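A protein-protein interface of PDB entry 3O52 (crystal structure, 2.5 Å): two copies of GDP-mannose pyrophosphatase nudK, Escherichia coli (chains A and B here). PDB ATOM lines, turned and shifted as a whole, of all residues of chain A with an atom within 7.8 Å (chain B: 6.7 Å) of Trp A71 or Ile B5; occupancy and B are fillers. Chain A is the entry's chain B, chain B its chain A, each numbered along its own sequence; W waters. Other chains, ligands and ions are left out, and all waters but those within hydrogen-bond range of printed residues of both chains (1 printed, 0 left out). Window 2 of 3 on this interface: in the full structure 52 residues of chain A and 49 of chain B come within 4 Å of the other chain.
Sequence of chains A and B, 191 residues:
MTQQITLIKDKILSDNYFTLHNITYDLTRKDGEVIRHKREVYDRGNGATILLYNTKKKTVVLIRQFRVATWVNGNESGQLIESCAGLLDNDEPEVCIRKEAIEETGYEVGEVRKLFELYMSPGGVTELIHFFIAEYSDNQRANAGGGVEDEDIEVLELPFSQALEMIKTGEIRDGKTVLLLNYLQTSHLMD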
ATOM      1  N   PHE A  66      23.880  21.782  20.285  1.00  0.00           N
ATOM      2  CA  PHE A  66      24.309  23.074  20.783  1.00  0.00           C
ATOM      3  C   PHE A  66      23.119  24.014  20.939  1.00  0.00           C
ATOM      4  O   PHE A  66      22.268  24.092  20.052  1.00  0.00           O
ATOM      5  CB  PHE A  66      25.370  23.690  19.875  1.00  0.00           C
ATOM      6  CG  PHE A  66      25.827  25.048  20.318  1.00  0.00           C
ATOM      7  CD1 PHE A  66      26.670  25.188  21.408  1.00  0.00           C
ATOM      8  CD2 PHE A  66      25.403  26.195  19.645  1.00  0.00           C
ATOM      9  CE1 PHE A  66      27.091  26.460  21.829  1.00  0.00           C
ATOM     10  CE2 PHE A  66      25.821  27.454  20.049  1.00  0.00           C
ATOM     11  CZ  PHE A  66      26.669  27.589  21.145  1.00  0.00           C
ATOM     12  N   ARG A  67      23.072  24.735  22.057  1.00  0.00           N
ATOM     13  CA  ARG A  67      22.010  25.702  22.324  1.00  0.00           C
ATOM     14  C   ARG A  67      22.544  27.053  22.797  1.00  0.00           C
ATOM     15  O   ARG A  67      22.907  27.202  23.969  1.00  0.00           O
ATOM     16  CB  ARG A  67      21.039  25.116  23.358  1.00  0.00           C
ATOM     17  CG  ARG A  67      20.180  23.986  22.863  1.00  0.00           C
ATOM     18  CD  ARG A  67      19.109  24.471  21.880  1.00  0.00           C
ATOM     19  NE  ARG A  67      17.860  23.721  22.044  1.00  0.00           N
ATOM     20  CZ  ARG A  67      16.877  23.655  21.143  1.00  0.00           C
ATOM     21  NH1 ARG A  67      16.988  24.258  19.960  1.00  0.00           N
ATOM     22  NH2 ARG A  67      15.778  22.945  21.430  1.00  0.00           N
ATOM     23  N   VAL A  68      22.584  28.041  21.894  1.00  0.00           N
ATOM     24  CA  VAL A  68      23.158  29.372  22.209  1.00  0.00           C
ATOM     25  C   VAL A  68      22.627  29.993  23.481  1.00  0.00           C
ATOM     26  O   VAL A  68      23.392  30.564  24.276  1.00  0.00           O
ATOM     27  CB  VAL A  68      22.891  30.465  21.154  1.00  0.00           C
ATOM     28  CG1 VAL A  68      24.150  30.823  20.434  1.00  0.00           C
ATOM     29  CG2 VAL A  68      21.693  30.157  20.246  1.00  0.00           C
ATOM     30  N   ALA A  69      21.312  29.926  23.636  1.00  0.00           N
ATOM     31  CA  ALA A  69      20.636  30.462  24.814  1.00  0.00           C
ATOM     32  C   ALA A  69      21.182  29.950  26.151  1.00  0.00           C
ATOM     33  O   ALA A  69      21.127  30.674  27.144  1.00  0.00           O
ATOM     34  CB  ALA A  69      19.138  30.213  24.732  1.00  0.00           C
ATOM     35  N   THR A  70      21.678  28.709  26.170  1.00  0.00           N
ATOM     36  CA  THR A  70      22.312  28.141  27.358  1.00  0.00           C
ATOM     37  C   THR A  70      23.804  28.494  27.369  1.00  0.00           C
ATOM     38  O   THR A  70      24.429  28.623  28.433  1.00  0.00           O
ATOM     39  CB  THR A  70      22.128  26.604  27.435  1.00  0.00           C
ATOM     40  OG1 THR A  70      22.917  25.966  26.419  1.00  0.00           O
ATOM     41  CG2 THR A  70      20.652  26.196  27.271  1.00  0.00           C
ATOM     42  N   TRP A  71      24.379  28.683  26.186  1.00  0.00           N
ATOM     43  CA  TRP A  71      25.801  28.975  26.084  1.00  0.00           C
ATOM     44  C   TRP A  71      26.153  30.340  26.691  1.00  0.00           C
ATOM     45  O   TRP A  71      27.224  30.536  27.277  1.00  0.00           O
ATOM     46  CB  TRP A  71      26.223  28.887  24.628  1.00  0.00           C
ATOM     47  CG  TRP A  71      27.675  29.040  24.421  1.00  0.00           C
ATOM     48  CD1 TRP A  71      28.672  28.185  24.826  1.00  0.00           C
ATOM     49  CD2 TRP A  71      28.319  30.115  23.739  1.00  0.00           C
ATOM     50  NE1 TRP A  71      29.899  28.681  24.432  1.00  0.00           N
ATOM     51  CE2 TRP A  71      29.706  29.858  23.762  1.00  0.00           C
ATOM     52  CE3 TRP A  71      27.856  31.268  23.100  1.00  0.00           C
ATOM     53  CZ2 TRP A  71      30.637  30.720  23.182  1.00  0.00           C
ATOM     54  CZ3 TRP A  71      28.788  32.133  22.518  1.00  0.00           C
ATOM     55  CH2 TRP A  71      30.157  31.855  22.566  1.00  0.00           C
ATOM     56  N   VAL A  72      25.236  31.285  26.565  1.00  0.00           N
ATOM     57  CA  VAL A  72      25.447  32.612  27.139  1.00  0.00           C
ATOM     58  C   VAL A  72      24.952  32.691  28.582  1.00  0.00           C
ATOM     59  O   VAL A  72      24.873  33.781  29.142  1.00  0.00           O
ATOM     60  CB  VAL A  72      24.742  33.703  26.308  1.00  0.00           C
ATOM     61  CG1 VAL A  72      25.349  33.801  24.906  1.00  0.00           C
ATOM     62  CG2 VAL A  72      23.260  33.451  26.233  1.00  0.00           C
ATOM     63  N   ASN A  73      24.600  31.535  29.166  1.00  0.00           N
ATOM     64  CA  ASN A  73      24.010  31.456  30.514  1.00  0.00           C
ATOM     65  C   ASN A  73      24.394  30.166  31.258  1.00  0.00           C
ATOM     66  O   ASN A  73      23.546  29.422  31.780  1.00  0.00           O
ATOM     67  CB  ASN A  73      22.490  31.679  30.455  1.00  0.00           C
ATOM     68  CG  ASN A  73      21.861  31.937  31.828  1.00  0.00           C
ATOM     69  OD1 ASN A  73      22.542  32.240  32.782  1.00  0.00           O
ATOM     70  ND2 ASN A  73      20.543  31.808  31.914  1.00  0.00           N
ATOM     71  N   GLY A  74      25.703  29.922  31.291  1.00  0.00           N
ATOM     72  CA  GLY A  74      26.304  28.874  32.132  1.00  0.00           C
ATOM     73  C   GLY A  74      26.383  27.453  31.616  1.00  0.00           C
ATOM     74  O   GLY A  74      26.778  26.559  32.377  1.00  0.00           O
ATOM     75  N   ASN A  75      25.975  27.192  30.371  1.00  0.00           N
ATOM     76  CA  ASN A  75      26.254  25.870  29.758  1.00  0.00           C
ATOM     77  C   ASN A  75      27.498  25.986  28.918  1.00  0.00           C
ATOM     78  O   ASN A  75      27.448  26.400  27.752  1.00  0.00           O
ATOM     79  CB  ASN A  75      25.112  25.382  28.892  1.00  0.00           C
ATOM     80  CG  ASN A  75      25.171  23.895  28.632  1.00  0.00           C
ATOM     81  OD1 ASN A  75      25.800  23.149  29.385  1.00  0.00           O
ATOM     82  ND2 ASN A  75      24.486  23.447  27.584  1.00  0.00           N
ATOM     83  N   GLU A  76      28.621  25.640  29.533  1.00  0.00           N
ATOM     84  CA  GLU A  76      29.937  26.002  29.028  1.00  0.00           C
ATOM     85  C   GLU A  76      30.180  25.566  27.571  1.00  0.00           C
ATOM     86  O   GLU A  76      30.652  26.372  26.762  1.00  0.00           O
ATOM     87  CB  GLU A  76      31.025  25.510  29.999  1.00  0.00           C
ATOM     88  CG  GLU A  76      30.855  26.061  31.450  1.00  0.00           C
ATOM     89  CD  GLU A  76      30.103  25.113  32.456  1.00  0.00           C
ATOM     90  OE1 GLU A  76      29.110  24.410  32.092  1.00  0.00           O
ATOM     91  OE2 GLU A  76      30.514  25.097  33.651  1.00  0.00           O
ATOM     92  N   SER A  77      29.809  24.319  27.247  1.00  0.00           N
ATOM     93  CA  SER A  77      29.942  23.760  25.891  1.00  0.00           C
ATOM     94  C   SER A  77      28.726  24.020  24.995  1.00  0.00           C
ATOM     95  O   SER A  77      28.791  23.799  23.787  1.00  0.00           O
ATOM     96  CB  SER A  77      30.205  22.247  25.950  1.00  0.00           C
ATOM     97  OG  SER A  77      29.006  21.499  26.153  1.00  0.00           O
ATOM     98  N   GLY A  78      27.619  24.456  25.591  1.00  0.00           N
ATOM     99  CA  GLY A  78      26.384  24.764  24.853  1.00  0.00           C
ATOM    100  C   GLY A  78      25.534  23.560  24.474  1.00  0.00           C
ATOM    101  O   GLY A  78      24.387  23.709  24.032  1.00  0.00           O
ATOM    102  N   GLN A  79      26.100  22.369  24.655  1.00  0.00           N
ATOM    103  CA  GLN A  79      25.425  21.114  24.341  1.00  0.00           C
ATOM    104  C   GLN A  79      24.417  20.819  25.419  1.00  0.00           C
ATOM    105  O   GLN A  79      24.712  20.935  26.594  1.00  0.00           O
ATOM    106  CB  GLN A  79      26.443  19.960  24.216  1.00  0.00           C
ATOM    107  CG  GLN A  79      27.541  20.214  23.152  1.00  0.00           C
ATOM    108  CD  GLN A  79      26.996  20.178  21.724  1.00  0.00           C
ATOM    109  OE1 GLN A  79      25.959  19.547  21.450  1.00  0.00           O
ATOM    110  NE2 GLN A  79      27.684  20.840  20.812  1.00  0.00           N
ATOM    111  N   GLN B   3      31.503  21.280  18.340  1.00  0.00           N
ATOM    112  CA  GLN B   3      32.712  21.510  19.192  1.00  0.00           C
ATOM    113  C   GLN B   3      33.082  23.008  19.267  1.00  0.00           C
ATOM    114  O   GLN B   3      32.609  23.721  20.156  1.00  0.00           O
ATOM    115  CB  GLN B   3      33.892  20.648  18.716  1.00  0.00           C
ATOM    116  CG  GLN B   3      35.132  20.713  19.613  1.00  0.00           C
ATOM    117  CD  GLN B   3      36.374  20.118  18.969  1.00  0.00           C
ATOM    118  OE1 GLN B   3      36.450  19.973  17.748  1.00  0.00           O
ATOM    119  NE2 GLN B   3      37.355  19.765  19.794  1.00  0.00           N
ATOM    120  N   GLN B   4      33.916  23.499  18.343  1.00  0.00           N
ATOM    121  CA  GLN B   4      34.322  24.916  18.384  1.00  0.00           C
ATOM    122  C   GLN B   4      33.146  25.860  18.063  1.00  0.00           C
ATOM    123  O   GLN B   4      32.526  25.770  16.992  1.00  0.00           O
ATOM    124  CB  GLN B   4      35.519  25.181  17.464  1.00  0.00           C
ATOM    125  CG  GLN B   4      36.100  26.628  17.472  1.00  0.00           C
ATOM    126  CD  GLN B   4      36.883  27.020  18.755  1.00  0.00           C
ATOM    127  OE1 GLN B   4      36.634  28.082  19.345  1.00  0.00           O
ATOM    128  NE2 GLN B   4      37.833  26.172  19.172  1.00  0.00           N
ATOM    129  N   ILE B   5      32.826  26.730  19.019  1.00  0.00           N
ATOM    130  CA  ILE B   5      31.844  27.799  18.837  1.00  0.00           C
ATOM    131  C   ILE B   5      32.484  29.189  18.966  1.00  0.00           C
ATOM    132  O   ILE B   5      33.165  29.476  19.936  1.00  0.00           O
ATOM    133  CB  ILE B   5      30.627  27.621  19.779  1.00  0.00           C
ATOM    134  CG1 ILE B   5      30.230  28.942  20.433  1.00  0.00           C
ATOM    135  CG2 ILE B   5      30.918  26.573  20.869  1.00  0.00           C
ATOM    136  CD1 ILE B   5      29.169  29.739  19.691  1.00  0.00           C
ATOM    137  N   THR B   6      32.264  30.041  17.964  1.00  0.00           N
ATOM    138  CA  THR B   6      32.820  31.406  17.946  1.00  0.00           C
ATOM    139  C   THR B   6      31.690  32.399  17.862  1.00  0.00           C
ATOM    140  O   THR B   6      30.857  32.299  16.967  1.00  0.00           O
ATOM    141  CB  THR B   6      33.751  31.661  16.730  1.00  0.00           C
ATOM    142  OG1 THR B   6      34.589  30.520  16.497  1.00  0.00           O
ATOM    143  CG2 THR B   6      34.620  32.891  16.964  1.00  0.00           C
ATOM    144  N   LEU B   7      31.660  33.358  18.784  1.00  0.00           N
ATOM    145  CA  LEU B   7      30.656  34.415  18.748  1.00  0.00           C
ATOM    146  C   LEU B   7      30.953  35.435  17.637  1.00  0.00           C
ATOM    147  O   LEU B   7      31.973  36.090  17.665  1.00  0.00           O
ATOM    148  CB  LEU B   7      30.575  35.115  20.106  1.00  0.00           C
ATOM    149  CG  LEU B   7      29.471  36.182  20.208  1.00  0.00           C
ATOM    150  CD1 LEU B   7      28.097  35.534  20.418  1.00  0.00           C
ATOM    151  CD2 LEU B   7      29.767  37.177  21.309  1.00  0.00           C
ATOM    152  N   ILE B   8      30.067  35.567  16.656  1.00  0.00           N
ATOM    153  CA  ILE B   8      30.300  36.532  15.565  1.00  0.00           C
ATOM    154  C   ILE B   8      29.614  37.877  15.831  1.00  0.00           C
ATOM    155  O   ILE B   8      30.221  38.910  15.639  1.00  0.00           O
ATOM    156  CB  ILE B   8      29.912  35.983  14.143  1.00  0.00           C
ATOM    157  CG1 ILE B   8      30.635  34.669  13.816  1.00  0.00           C
ATOM    158  CG2 ILE B   8      30.211  37.003  13.060  1.00  0.00           C
ATOM    159  CD1 ILE B   8      32.148  34.787  13.727  1.00  0.00           C
ATOM    160  N   ILE B  23      21.848  36.585  17.885  1.00  0.00           N
ATOM    161  CA  ILE B  23      23.245  36.156  18.003  1.00  0.00           C
ATOM    162  C   ILE B  23      23.666  35.464  16.731  1.00  0.00           C
ATOM    163  O   ILE B  23      23.063  34.459  16.363  1.00  0.00           O
ATOM    164  CB  ILE B  23      23.504  35.219  19.231  1.00  0.00           C
ATOM    165  CG1 ILE B  23      23.721  36.046  20.485  1.00  0.00           C
ATOM    166  CG2 ILE B  23      24.795  34.435  19.065  1.00  0.00           C
ATOM    167  CD1 ILE B  23      22.505  36.267  21.236  1.00  0.00           C
ATOM    168  N   THR B  24      24.669  36.019  16.058  1.00  0.00           N
ATOM    169  CA  THR B  24      25.315  35.362  14.934  1.00  0.00           C
ATOM    170  C   THR B  24      26.510  34.568  15.500  1.00  0.00           C
ATOM    171  O   THR B  24      27.349  35.138  16.225  1.00  0.00           O
ATOM    172  CB  THR B  24      25.800  36.391  13.846  1.00  0.00           C
ATOM    173  OG1 THR B  24      24.744  37.319  13.495  1.00  0.00           O
ATOM    174  CG2 THR B  24      26.278  35.668  12.585  1.00  0.00           C
ATOM    175  N   TYR B  25      26.579  33.263  15.194  1.00  0.00           N
ATOM    176  CA  TYR B  25      27.678  32.412  15.681  1.00  0.00           C
ATOM    177  C   TYR B  25      28.071  31.310  14.701  1.00  0.00           C
ATOM    178  O   TYR B  25      27.283  30.928  13.833  1.00  0.00           O
ATOM    179  CB  TYR B  25      27.354  31.823  17.060  1.00  0.00           C
ATOM    180  CG  TYR B  25      26.245  30.799  17.042  1.00  0.00           C
ATOM    181  CD1 TYR B  25      26.519  29.441  16.824  1.00  0.00           C
ATOM    182  CD2 TYR B  25      24.928  31.175  17.232  1.00  0.00           C
ATOM    183  CE1 TYR B  25      25.486  28.484  16.781  1.00  0.00           C
ATOM    184  CE2 TYR B  25      23.900  30.225  17.203  1.00  0.00           C
ATOM    185  CZ  TYR B  25      24.191  28.886  16.984  1.00  0.00           C
ATOM    186  OH  TYR B  25      23.181  27.961  16.944  1.00  0.00           O
ATOM    187  N   ASP B  26      29.283  30.790  14.882  1.00  0.00           N
ATOM    188  CA  ASP B  26      29.887  29.819  13.986  1.00  0.00           C
ATOM    189  C   ASP B  26      30.188  28.478  14.670  1.00  0.00           C
ATOM    190  O   ASP B  26      30.878  28.446  15.687  1.00  0.00           O
ATOM    191  CB  ASP B  26      31.186  30.405  13.419  1.00  0.00           C
ATOM    192  CG  ASP B  26      30.955  31.289  12.196  1.00  0.00           C
ATOM    193  OD1 ASP B  26      29.812  31.321  11.696  1.00  0.00           O
ATOM    194  OD2 ASP B  26      31.922  31.935  11.732  1.00  0.00           O
ATOM    195  N   LEU B  27      29.675  27.382  14.114  1.00  0.00           N
ATOM    196  CA  LEU B  27      30.055  26.050  14.564  1.00  0.00           C
ATOM    197  C   LEU B  27      30.969  25.393  13.562  1.00  0.00           C
ATOM    198  O   LEU B  27      30.846  25.627  12.372  1.00  0.00           O
ATOM    199  CB  LEU B  27      28.851  25.138  14.761  1.00  0.00           C
ATOM    200  CG  LEU B  27      27.938  25.295  15.964  1.00  0.00           C
ATOM    201  CD1 LEU B  27      26.934  24.168  15.964  1.00  0.00           C
ATOM    202  CD2 LEU B  27      28.735  25.302  17.241  1.00  0.00           C
ATOM    203  N   THR B  28      31.884  24.564  14.051  1.00  0.00           N
ATOM    204  CA  THR B  28      32.720  23.742  13.184  1.00  0.00           C
ATOM    205  C   THR B  28      32.180  22.313  13.233  1.00  0.00           C
ATOM    206  O   THR B  28      31.820  21.807  14.305  1.00  0.00           O
ATOM    207  CB  THR B  28      34.154  23.781  13.640  1.00  0.00           C
ATOM    208  OG1 THR B  28      34.162  23.634  15.068  1.00  0.00           O
ATOM    209  CG2 THR B  28      34.793  25.118  13.264  1.00  0.00           C
ATOM    210  N   TYR B 119      16.827  24.686  32.496  1.00  0.00           N
ATOM    211  CA  TYR B 119      16.427  25.618  31.440  1.00  0.00           C
ATOM    212  C   TYR B 119      15.010  25.248  31.032  1.00  0.00           C
ATOM    213  O   TYR B 119      14.747  24.105  30.609  1.00  0.00           O
ATOM    214  CB  TYR B 119      17.363  25.509  30.233  1.00  0.00           C
ATOM    215  CG  TYR B 119      18.789  25.954  30.525  1.00  0.00           C
ATOM    216  CD1 TYR B 119      19.134  27.295  30.527  1.00  0.00           C
ATOM    217  CD2 TYR B 119      19.788  25.016  30.800  1.00  0.00           C
ATOM    218  CE1 TYR B 119      20.428  27.691  30.790  1.00  0.00           C
ATOM    219  CE2 TYR B 119      21.072  25.392  31.062  1.00  0.00           C
ATOM    220  CZ  TYR B 119      21.397  26.740  31.062  1.00  0.00           C
ATOM    221  OH  TYR B 119      22.720  27.124  31.328  1.00  0.00           O
HETATM  222  O   HOH W   1      21.696  26.867  19.316  1.00  0.00           O
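Among the printed residues, merely in contact across the chains: Phe A66 with Ile B5 (3.6 Å), Phe A66 with Tyr B25 (3.4 Å), Val A68 with Ile B23 (3.9 Å), Val A68 with Tyr B25 (3.3 Å), Thr A70 with Tyr B119 (3.7 Å), Trp A71 with Ile B5 (3.3 Å) and Gly A74 with Tyr B119 (3.7 Å).
Printed residues of chain B that touch a printed residue of chain A: Ile B5, Ile B23, Tyr B25 and Tyr B119. Hydrophobic or aromatic side chains of chain B that line the printed part of chain A: Ile B5, Ile B23, Tyr B25 and Tyr B119. Of the 14 printed residues of chain A, 7 touch a printed residue of chain B. Among the printed residues, 9 pairs touch across the chains.
No position is printed for both chains. Of the 9 pairs that touch across the chains among the printed residues, none has its exchanged pair printed and touching as well.
Of the printed residues of chain B, Thr A70 touches Tyr B119 (3.7 Å). Of the printed residues of chain B, Gly A74 touches Tyr B119. Of chain A, only Phe A66 (3.6 Å) and Trp A71 (3.3 Å) come within 4 Å of Ile B5. Of the printed residues of chain A, Ile B23 touches Val A68 (3.9 Å). Asp B26 touches none of the printed residues of chain A. The nearest residue of chain B that does not touch Trp A71 is Leu B7 (4.1 Å). The nearest printed residue of chain B that does not touch Thr A70 is Ile B23 (9.1 Å).
The backbone NH (N) of Phe A66 lies within hydrogen-bond range of the side-chain amide oxygen (OE1) of Gln A79, 3.3 Å away. O of Arg A67 lies within hydrogen-bond range of OG1 of Thr A70, 2.7 Å away. O of Thr A70 lies within hydrogen-bond range of N of Asn A75, at 2.9 Å. The backbone carbonyl oxygen of Glu A76 lies close to the indole nitrogen of Trp A71. The backbone carbonyl oxygen (O) of Gln A79 sits at hydrogen-bond distance from the side-chain amide nitrogen (ND2) of Asn A75, 2.7 Å away.
Water W1 lies within hydrogen-bond range of O of Phe A66 (2.9 Å), N of Val A68 (3.0 Å) and OH of Tyr B25 (3.0 Å).
OH of Tyr B119 sits at hydrogen-bond distance from O of Asn A73 (2.5 Å). N of Asn A75 is in hydrogen-bond range of OH of Tyr B119 (3.4 Å).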
